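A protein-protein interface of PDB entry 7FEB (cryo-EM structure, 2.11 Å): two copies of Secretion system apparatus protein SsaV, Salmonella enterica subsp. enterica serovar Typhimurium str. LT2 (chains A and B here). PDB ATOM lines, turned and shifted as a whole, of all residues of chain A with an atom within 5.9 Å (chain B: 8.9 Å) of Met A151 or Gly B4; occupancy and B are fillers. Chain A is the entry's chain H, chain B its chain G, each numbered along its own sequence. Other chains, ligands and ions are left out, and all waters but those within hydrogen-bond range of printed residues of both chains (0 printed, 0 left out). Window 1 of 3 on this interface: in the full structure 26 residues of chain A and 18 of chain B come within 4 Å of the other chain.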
ATOM      1  N   PHE A  33      -3.633  13.952  26.748  1.00  0.00           N
ATOM      2  CA  PHE A  33      -4.282  15.253  26.862  1.00  0.00           C
ATOM      3  C   PHE A  33      -5.728  15.188  26.393  1.00  0.00           C
ATOM      4  O   PHE A  33      -6.621  15.758  27.030  1.00  0.00           O
ATOM      5  CB  PHE A  33      -3.519  16.310  26.067  1.00  0.00           C
ATOM      6  CG  PHE A  33      -4.244  17.621  25.966  1.00  0.00           C
ATOM      7  CD1 PHE A  33      -4.328  18.465  27.061  1.00  0.00           C
ATOM      8  CD2 PHE A  33      -4.856  18.005  24.783  1.00  0.00           C
ATOM      9  CE1 PHE A  33      -5.001  19.669  26.975  1.00  0.00           C
ATOM     10  CE2 PHE A  33      -5.529  19.207  24.693  1.00  0.00           C
ATOM     11  CZ  PHE A  33      -5.602  20.039  25.789  1.00  0.00           C
ATOM     12  N   TYR A 146      -2.120  28.286  33.339  1.00  0.00           N
ATOM     13  CA  TYR A 146      -1.905  28.041  31.916  1.00  0.00           C
ATOM     14  C   TYR A 146      -3.209  27.689  31.211  1.00  0.00           C
ATOM     15  O   TYR A 146      -3.491  28.196  30.117  1.00  0.00           O
ATOM     16  CB  TYR A 146      -0.879  26.925  31.723  1.00  0.00           C
ATOM     17  CG  TYR A 146      -0.846  26.376  30.316  1.00  0.00           C
ATOM     18  CD1 TYR A 146      -0.130  27.021  29.319  1.00  0.00           C
ATOM     19  CD2 TYR A 146      -1.540  25.222  29.983  1.00  0.00           C
ATOM     20  CE1 TYR A 146      -0.102  26.529  28.032  1.00  0.00           C
ATOM     21  CE2 TYR A 146      -1.522  24.725  28.700  1.00  0.00           C
ATOM     22  CZ  TYR A 146      -0.801  25.380  27.727  1.00  0.00           C
ATOM     23  OH  TYR A 146      -0.776  24.885  26.446  1.00  0.00           O
ATOM     24  N   LEU A 147      -4.014  26.816  31.818  1.00  0.00           N
ATOM     25  CA  LEU A 147      -5.286  26.437  31.208  1.00  0.00           C
ATOM     26  C   LEU A 147      -6.228  27.631  31.111  1.00  0.00           C
ATOM     27  O   LEU A 147      -6.928  27.799  30.107  1.00  0.00           O
ATOM     28  CB  LEU A 147      -5.937  25.302  31.998  1.00  0.00           C
ATOM     29  CG  LEU A 147      -5.318  23.913  31.843  1.00  0.00           C
ATOM     30  CD1 LEU A 147      -5.987  22.924  32.777  1.00  0.00           C
ATOM     31  CD2 LEU A 147      -5.398  23.440  30.404  1.00  0.00           C
ATOM     32  N   MET A 148      -6.254  28.474  32.144  1.00  0.00           N
ATOM     33  CA  MET A 148      -7.117  29.649  32.120  1.00  0.00           C
ATOM     34  C   MET A 148      -6.653  30.659  31.077  1.00  0.00           C
ATOM     35  O   MET A 148      -7.480  31.297  30.416  1.00  0.00           O
ATOM     36  CB  MET A 148      -7.170  30.287  33.504  1.00  0.00           C
ATOM     37  CG  MET A 148      -8.196  29.662  34.426  1.00  0.00           C
ATOM     38  SD  MET A 148      -7.686  29.688  36.150  1.00  0.00           S
ATOM     39  CE  MET A 148      -8.195  31.336  36.616  1.00  0.00           C
ATOM     40  N   ASN A 149      -5.339  30.826  30.924  1.00  0.00           N
ATOM     41  CA  ASN A 149      -4.818  31.714  29.891  1.00  0.00           C
ATOM     42  C   ASN A 149      -5.152  31.197  28.501  1.00  0.00           C
ATOM     43  O   ASN A 149      -5.475  31.980  27.600  1.00  0.00           O
ATOM     44  CB  ASN A 149      -3.306  31.879  30.050  1.00  0.00           C
ATOM     45  CG  ASN A 149      -2.938  32.785  31.205  1.00  0.00           C
ATOM     46  OD1 ASN A 149      -3.782  33.493  31.749  1.00  0.00           O
ATOM     47  ND2 ASN A 149      -1.668  32.768  31.585  1.00  0.00           N
ATOM     48  N   ALA A 150      -5.066  29.879  28.304  1.00  0.00           N
ATOM     49  CA  ALA A 150      -5.457  29.301  27.024  1.00  0.00           C
ATOM     50  C   ALA A 150      -6.946  29.487  26.764  1.00  0.00           C
ATOM     51  O   ALA A 150      -7.360  29.718  25.622  1.00  0.00           O
ATOM     52  CB  ALA A 150      -5.084  27.820  26.983  1.00  0.00           C
ATOM     53  N   MET A 151      -7.768  29.388  27.809  1.00  0.00           N
ATOM     54  CA  MET A 151      -9.210  29.522  27.655  1.00  0.00           C
ATOM     55  C   MET A 151      -9.648  30.952  27.367  1.00  0.00           C
ATOM     56  O   MET A 151     -10.806  31.160  26.996  1.00  0.00           O
ATOM     57  CB  MET A 151      -9.917  29.010  28.910  1.00  0.00           C
ATOM     58  CG  MET A 151     -10.208  27.520  28.893  1.00  0.00           C
ATOM     59  SD  MET A 151     -11.454  27.029  27.691  1.00  0.00           S
ATOM     60  CE  MET A 151     -12.956  27.329  28.617  1.00  0.00           C
ATOM     61  N   GLU A 152      -8.761  31.934  27.517  1.00  0.00           N
ATOM     62  CA  GLU A 152      -9.124  33.329  27.311  1.00  0.00           C
ATOM     63  C   GLU A 152      -9.246  33.712  25.843  1.00  0.00           C
ATOM     64  O   GLU A 152      -9.742  34.802  25.545  1.00  0.00           O
ATOM     65  CB  GLU A 152      -8.103  34.247  27.986  1.00  0.00           C
ATOM     66  CG  GLU A 152      -8.343  34.458  29.467  1.00  0.00           C
ATOM     67  CD  GLU A 152      -7.245  35.264  30.127  1.00  0.00           C
ATOM     68  OE1 GLU A 152      -6.365  35.773  29.404  1.00  0.00           O
ATOM     69  OE2 GLU A 152      -7.260  35.390  31.367  1.00  0.00           O
ATOM     70  N   LYS A 153      -8.802  32.854  24.922  1.00  0.00           N
ATOM     71  CA  LYS A 153      -8.933  33.162  23.502  1.00  0.00           C
ATOM     72  C   LYS A 153     -10.398  33.220  23.083  1.00  0.00           C
ATOM     73  O   LYS A 153     -10.830  34.174  22.427  1.00  0.00           O
ATOM     74  CB  LYS A 153      -8.175  32.130  22.671  1.00  0.00           C
ATOM     75  CG  LYS A 153      -7.627  32.671  21.364  1.00  0.00           C
ATOM     76  CD  LYS A 153      -7.420  31.559  20.350  1.00  0.00           C
ATOM     77  CE  LYS A 153      -8.512  31.565  19.296  1.00  0.00           C
ATOM     78  NZ  LYS A 153      -8.646  30.239  18.629  1.00  0.00           N
ATOM     79  N   ASN A 154     -11.179  32.209  23.461  1.00  0.00           N
ATOM     80  CA  ASN A 154     -12.579  32.127  23.076  1.00  0.00           C
ATOM     81  C   ASN A 154     -13.544  32.345  24.231  1.00  0.00           C
ATOM     82  O   ASN A 154     -14.746  32.489  23.986  1.00  0.00           O
ATOM     83  CB  ASN A 154     -12.872  30.764  22.431  1.00  0.00           C
ATOM     84  CG  ASN A 154     -12.114  30.556  21.137  1.00  0.00           C
ATOM     85  OD1 ASN A 154     -11.748  31.514  20.459  1.00  0.00           O
ATOM     86  ND2 ASN A 154     -11.877  29.300  20.786  1.00  0.00           N
ATOM     87  N   TYR A 155     -13.063  32.370  25.471  1.00  0.00           N
ATOM     88  CA  TYR A 155     -13.925  32.469  26.644  1.00  0.00           C
ATOM     89  C   TYR A 155     -13.364  33.488  27.629  1.00  0.00           C
ATOM     90  O   TYR A 155     -13.253  33.233  28.828  1.00  0.00           O
ATOM     91  CB  TYR A 155     -14.094  31.104  27.306  1.00  0.00           C
ATOM     92  CG  TYR A 155     -14.604  30.033  26.376  1.00  0.00           C
ATOM     93  CD1 TYR A 155     -15.963  29.890  26.133  1.00  0.00           C
ATOM     94  CD2 TYR A 155     -13.729  29.164  25.739  1.00  0.00           C
ATOM     95  CE1 TYR A 155     -16.436  28.915  25.286  1.00  0.00           C
ATOM     96  CE2 TYR A 155     -14.194  28.182  24.889  1.00  0.00           C
ATOM     97  CZ  TYR A 155     -15.549  28.063  24.666  1.00  0.00           C
ATOM     98  OH  TYR A 155     -16.022  27.090  23.821  1.00  0.00           O
ATOM     99  N   SER A 156     -13.000  34.666  27.120  1.00  0.00           N
ATOM    100  CA  SER A 156     -12.425  35.699  27.977  1.00  0.00           C
ATOM    101  C   SER A 156     -13.396  36.114  29.078  1.00  0.00           C
ATOM    102  O   SER A 156     -13.003  36.257  30.243  1.00  0.00           O
ATOM    103  CB  SER A 156     -12.022  36.906  27.131  1.00  0.00           C
ATOM    104  OG  SER A 156     -11.123  37.744  27.831  1.00  0.00           O
ATOM    105  N   LEU A 158     -15.881  34.332  30.332  1.00  0.00           N
ATOM    106  CA  LEU A 158     -16.046  33.220  31.263  1.00  0.00           C
ATOM    107  C   LEU A 158     -14.892  33.151  32.258  1.00  0.00           C
ATOM    108  O   LEU A 158     -15.108  32.967  33.461  1.00  0.00           O
ATOM    109  CB  LEU A 158     -16.170  31.912  30.482  1.00  0.00           C
ATOM    110  CG  LEU A 158     -16.382  30.611  31.254  1.00  0.00           C
ATOM    111  CD1 LEU A 158     -17.768  30.568  31.859  1.00  0.00           C
ATOM    112  CD2 LEU A 158     -16.157  29.416  30.348  1.00  0.00           C
ATOM    113  N   VAL A 159     -13.659  33.304  31.773  1.00  0.00           N
ATOM    114  CA  VAL A 159     -12.497  33.277  32.656  1.00  0.00           C
ATOM    115  C   VAL A 159     -12.521  34.461  33.613  1.00  0.00           C
ATOM    116  O   VAL A 159     -12.213  34.323  34.804  1.00  0.00           O
ATOM    117  CB  VAL A 159     -11.201  33.234  31.823  1.00  0.00           C
ATOM    118  CG1 VAL A 159      -9.985  33.482  32.703  1.00  0.00           C
ATOM    119  CG2 VAL A 159     -11.078  31.903  31.108  1.00  0.00           C
ATOM    120  N   ARG A 186     -11.181  18.037  30.247  1.00  0.00           N
ATOM    121  CA  ARG A 186     -11.143  18.513  28.869  1.00  0.00           C
ATOM    122  C   ARG A 186     -12.193  19.593  28.627  1.00  0.00           C
ATOM    123  O   ARG A 186     -11.931  20.580  27.931  1.00  0.00           O
ATOM    124  CB  ARG A 186     -11.344  17.338  27.912  1.00  0.00           C
ATOM    125  CG  ARG A 186     -11.145  17.672  26.447  1.00  0.00           C
ATOM    126  CD  ARG A 186      -9.692  17.961  26.135  1.00  0.00           C
ATOM    127  NE  ARG A 186      -9.473  18.150  24.707  1.00  0.00           N
ATOM    128  CZ  ARG A 186      -9.236  19.319  24.130  1.00  0.00           C
ATOM    129  NH1 ARG A 186      -9.184  20.438  24.832  1.00  0.00           N
ATOM    130  NH2 ARG A 186      -9.043  19.367  22.817  1.00  0.00           N
ATOM    131  N   LEU A 188     -13.400  22.393  29.828  1.00  0.00           N
ATOM    132  CA  LEU A 188     -13.158  23.485  30.764  1.00  0.00           C
ATOM    133  C   LEU A 188     -14.307  24.484  30.781  1.00  0.00           C
ATOM    134  O   LEU A 188     -14.556  25.117  31.811  1.00  0.00           O
ATOM    135  CB  LEU A 188     -11.849  24.193  30.419  1.00  0.00           C
ATOM    136  CG  LEU A 188     -10.566  23.451  30.794  1.00  0.00           C
ATOM    137  CD1 LEU A 188      -9.352  24.192  30.267  1.00  0.00           C
ATOM    138  CD2 LEU A 188     -10.477  23.261  32.298  1.00  0.00           C
ATOM    139  N   ARG A 189     -14.998  24.613  29.644  1.00  0.00           N
ATOM    140  CA  ARG A 189     -16.141  25.559  29.515  1.00  0.00           C
ATOM    141  C   ARG A 189     -17.242  25.176  30.510  1.00  0.00           C
ATOM    142  O   ARG A 189     -17.746  26.079  31.208  1.00  0.00           O
ATOM    143  CB  ARG A 189     -16.674  25.558  28.079  1.00  0.00           C
ATOM    144  CG  ARG A 189     -17.376  26.846  27.676  1.00  0.00           C
ATOM    145  CD  ARG A 189     -18.475  26.611  26.656  1.00  0.00           C
ATOM    146  NE  ARG A 189     -19.570  25.815  27.193  1.00  0.00           N
ATOM    147  CZ  ARG A 189     -20.854  26.142  27.101  1.00  0.00           C
ATOM    148  NH1 ARG A 189     -21.211  27.257  26.488  1.00  0.00           N
ATOM    149  NH2 ARG A 189     -21.776  25.353  27.622  1.00  0.00           N
ATOM    150  N   PHE A 192     -15.957  25.503  34.293  1.00  0.00           N
ATOM    151  CA  PHE A 192     -15.940  26.898  34.718  1.00  0.00           C
ATOM    152  C   PHE A 192     -17.352  27.432  34.910  1.00  0.00           C
ATOM    153  O   PHE A 192     -17.611  28.187  35.853  1.00  0.00           O
ATOM    154  CB  PHE A 192     -15.174  27.754  33.707  1.00  0.00           C
ATOM    155  CG  PHE A 192     -13.695  27.484  33.673  1.00  0.00           C
ATOM    156  CD1 PHE A 192     -13.098  26.666  34.616  1.00  0.00           C
ATOM    157  CD2 PHE A 192     -12.903  28.051  32.692  1.00  0.00           C
ATOM    158  CE1 PHE A 192     -11.743  26.421  34.580  1.00  0.00           C
ATOM    159  CE2 PHE A 192     -11.546  27.806  32.652  1.00  0.00           C
ATOM    160  CZ  PHE A 192     -10.966  26.991  33.598  1.00  0.00           C
ATOM    161  N   MET B   1      -2.339  20.245  21.676  1.00  0.00           N
ATOM    162  CA  MET B   1      -2.908  20.491  22.995  1.00  0.00           C
ATOM    163  C   MET B   1      -3.483  21.899  23.098  1.00  0.00           C
ATOM    164  O   MET B   1      -2.798  22.830  23.517  1.00  0.00           O
ATOM    165  CB  MET B   1      -1.855  20.278  24.084  1.00  0.00           C
ATOM    166  CG  MET B   1      -1.234  18.892  24.098  1.00  0.00           C
ATOM    167  SD  MET B   1      -0.151  18.654  25.520  1.00  0.00           S
ATOM    168  CE  MET B   1      -0.214  16.876  25.708  1.00  0.00           C
ATOM    169  N   VAL B   2      -4.744  22.049  22.706  1.00  0.00           N
ATOM    170  CA  VAL B   2      -5.459  23.317  22.773  1.00  0.00           C
ATOM    171  C   VAL B   2      -6.556  23.177  23.827  1.00  0.00           C
ATOM    172  O   VAL B   2      -7.533  22.444  23.607  1.00  0.00           O
ATOM    173  CB  VAL B   2      -6.041  23.714  21.411  1.00  0.00           C
ATOM    174  CG1 VAL B   2      -6.690  25.085  21.493  1.00  0.00           C
ATOM    175  CG2 VAL B   2      -4.957  23.698  20.346  1.00  0.00           C
ATOM    176  N   PRO B   3      -6.435  23.833  24.980  1.00  0.00           N
ATOM    177  CA  PRO B   3      -7.487  23.737  25.999  1.00  0.00           C
ATOM    178  C   PRO B   3      -8.820  24.257  25.482  1.00  0.00           C
ATOM    179  O   PRO B   3      -8.879  25.217  24.712  1.00  0.00           O
ATOM    180  CB  PRO B   3      -6.949  24.601  27.143  1.00  0.00           C
ATOM    181  CG  PRO B   3      -5.470  24.605  26.945  1.00  0.00           C
ATOM    182  CD  PRO B   3      -5.265  24.585  25.462  1.00  0.00           C
ATOM    183  N   GLY B   4      -9.895  23.609  25.919  1.00  0.00           N
ATOM    184  CA  GLY B   4     -11.223  23.927  25.438  1.00  0.00           C
ATOM    185  C   GLY B   4     -11.698  22.944  24.389  1.00  0.00           C
ATOM    186  O   GLY B   4     -11.220  22.965  23.251  1.00  0.00           O
ATOM    187  N   ALA B   5     -12.631  22.075  24.763  1.00  0.00           N
ATOM    188  CA  ALA B   5     -13.143  21.077  23.837  1.00  0.00           C
ATOM    189  C   ALA B   5     -13.832  21.738  22.649  1.00  0.00           C
ATOM    190  O   ALA B   5     -14.459  22.794  22.772  1.00  0.00           O
ATOM    191  CB  ALA B   5     -14.115  20.140  24.555  1.00  0.00           C
ATOM    192  N   CYS B   6     -13.698  21.111  21.486  1.00  0.00           N
ATOM    193  CA  CYS B   6     -14.372  21.602  20.288  1.00  0.00           C
ATOM    194  C   CYS B   6     -15.881  21.473  20.464  1.00  0.00           C
ATOM    195  O   CYS B   6     -16.368  20.385  20.786  1.00  0.00           O
ATOM    196  CB  CYS B   6     -13.912  20.822  19.059  1.00  0.00           C
ATOM    197  SG  CYS B   6     -14.791  21.232  17.537  1.00  0.00           S
ATOM    198  N   PRO B   7     -16.649  22.544  20.251  1.00  0.00           N
ATOM    199  CA  PRO B   7     -18.077  22.498  20.620  1.00  0.00           C
ATOM    200  C   PRO B   7     -18.904  21.490  19.833  1.00  0.00           C
ATOM    201  O   PRO B   7     -19.657  20.718  20.436  1.00  0.00           O
ATOM    202  CB  PRO B   7     -18.540  23.941  20.369  1.00  0.00           C
ATOM    203  CG  PRO B   7     -17.295  24.760  20.404  1.00  0.00           C
ATOM    204  CD  PRO B   7     -16.227  23.890  19.833  1.00  0.00           C
ATOM    205  N   TYR B  60     -18.957  19.187  22.519  1.00  0.00           N
ATOM    206  CA  TYR B  60     -17.752  19.382  23.325  1.00  0.00           C
ATOM    207  C   TYR B  60     -16.993  18.067  23.485  1.00  0.00           C
ATOM    208  O   TYR B  60     -16.560  17.699  24.578  1.00  0.00           O
ATOM    209  CB  TYR B  60     -18.094  20.018  24.673  1.00  0.00           C
ATOM    210  CG  TYR B  60     -18.766  21.362  24.512  1.00  0.00           C
ATOM    211  CD1 TYR B  60     -18.031  22.489  24.178  1.00  0.00           C
ATOM    212  CD2 TYR B  60     -20.140  21.497  24.657  1.00  0.00           C
ATOM    213  CE1 TYR B  60     -18.642  23.716  24.011  1.00  0.00           C
ATOM    214  CE2 TYR B  60     -20.758  22.719  24.493  1.00  0.00           C
ATOM    215  CZ  TYR B  60     -20.005  23.824  24.171  1.00  0.00           C
ATOM    216  OH  TYR B  60     -20.616  25.044  24.008  1.00  0.00           O
ATOM    217  N   GLN B  61     -16.862  17.346  22.370  1.00  0.00           N
ATOM    218  CA  GLN B  61     -16.086  16.115  22.238  1.00  0.00           C
ATOM    219  C   GLN B  61     -16.652  14.957  23.051  1.00  0.00           C
ATOM    220  O   GLN B  61     -15.957  13.965  23.279  1.00  0.00           O
ATOM    221  CB  GLN B  61     -14.614  16.347  22.595  1.00  0.00           C
ATOM    222  CG  GLN B  61     -13.887  17.211  21.581  1.00  0.00           C
ATOM    223  CD  GLN B  61     -12.459  17.508  21.974  1.00  0.00           C
ATOM    224  OE1 GLN B  61     -11.863  18.473  21.501  1.00  0.00           O
ATOM    225  NE2 GLN B  61     -11.899  16.676  22.842  1.00  0.00           N
ATOM    226  N   GLN B 142     -20.164  33.175  28.401  1.00  0.00           N
ATOM    227  CA  GLN B 142     -19.508  33.717  27.213  1.00  0.00           C
ATOM    228  C   GLN B 142     -20.512  34.012  26.104  1.00  0.00           C
ATOM    229  O   GLN B 142     -20.418  35.042  25.427  1.00  0.00           O
ATOM    230  CB  GLN B 142     -18.434  32.747  26.718  1.00  0.00           C
ATOM    231  CG  GLN B 142     -17.602  33.282  25.568  1.00  0.00           C
ATOM    232  CD  GLN B 142     -16.826  34.525  25.947  1.00  0.00           C
ATOM    233  OE1 GLN B 142     -16.302  34.627  27.052  1.00  0.00           O
ATOM    234  NE2 GLN B 142     -16.750  35.478  25.033  1.00  0.00           N
ATOM    235  N   GLU B 143     -21.479  33.119  25.901  1.00  0.00           N
ATOM    236  CA  GLU B 143     -22.483  33.334  24.867  1.00  0.00           C
ATOM    237  C   GLU B 143     -23.408  34.490  25.230  1.00  0.00           C
ATOM    238  O   GLU B 143     -23.814  35.269  24.360  1.00  0.00           O
ATOM    239  CB  GLU B 143     -23.269  32.045  24.641  1.00  0.00           C
ATOM    240  CG  GLU B 143     -22.444  30.918  24.023  1.00  0.00           C
ATOM    241  CD  GLU B 143     -21.475  30.267  25.005  1.00  0.00           C
ATOM    242  OE1 GLU B 143     -21.833  30.106  26.189  1.00  0.00           O
ATOM    243  OE2 GLU B 143     -20.351  29.922  24.590  1.00  0.00           O
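Tyr A146 touches none of the printed residues of chain B. Of chain B, only Pro B3 (3.2 Å) comes within 4 Å of Ala A150. Met A151 touches one residue of chain B. Printed residues of chain B within 4 Å of Leu A158: Gln B142 (3.3 Å). Printed residues of chain A within 4 Å of Val B2: Phe A33 (3.6 Å) and Arg A186 (2.9 Å). Of the printed residues of chain A, Gly B4 touches Met A151 (3.8 Å) and Arg A186 (3.4 Å). Of the printed residues of chain A, Gln B61 touches Arg A186 (3.2 Å). The nearest residue of chain B that does not touch Met A151 is Pro B3 (4.3 Å). The nearest printed residue of chain A that does not touch Ala B5 is Tyr A155 (4.7 Å).
No position is printed for both chains. Of the 18 pairs that touch across the chains among the printed residues, none has its exchanged pair printed and touching as well.
Phe A33 touches Met B1 (CB to CE, 3.4 Å). N of Val B2 touches CE2 of Phe A33, 3.6 Å away. N of Pro B3 touches CZ of Phe A33, 3.97 Å away. Leu A147 touches Pro B3. CB of Ala A150 touches CG of Pro B3, 3.2 Å away. Met A151 touches Gly B4. Asn A154 touches Gln B142 (O to CG, 3.4 Å). CA of Pro B3 touches NH1 of Arg A186, 3.9 Å away. O of Arg A186 touches N of Ala B5, at 3.6 Å. Leu A188 touches Pro B3 (CD1 to CB, 3.96 Å).
OE1 of Gln B142 lies within hydrogen-bond range of N of Ser A156, at 3.3 Å. The guanidinium group (NH1) of Arg A189 lies within salt-bridge range of the side-chain carboxylate (OE1) of Glu B143, 2.9 Å away. OE1 of Gln B142 is in hydrogen-bond range of N of Leu A158, at 3.3 Å. The guanidinium group (NH1) of Arg A186 sits close to the backbone NH (N) of Gly B4 (3.4 Å). O of Val B2 lies within hydrogen-bond range of NH1 of Arg A186 (2.9 Å). The guanidinium group of Arg A189 lies close to the side-chain hydroxyl of Tyr B60, at 3.4 Å. The side-chain amide oxygen (OE1) of Gln B61 is in hydrogen-bond range of the guanidinium group (NH2) of Arg A186.
The backbone carbonyl oxygen (O) of Cys B6 sits close to the backbone NH (N) of Tyr B60 (3.3 Å). The backbone carbonyl oxygen (O) of Pro B7 lies within hydrogen-bond range of the backbone NH (N) of Tyr B60 (2.7 Å). The side-chain amide oxygen of Gln B61 sits at hydrogen-bond distance from the backbone NH of Cys B6, 3.2 Å away.
Of the 18 printed residues of chain A, 11 touch a printed residue of chain B. Hydrophobic or aromatic side chains of chain A within 4 Å of the printed part of chain B: Phe A33, Leu A147, Ala A150, Met A151, Tyr A155 and Leu A188.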
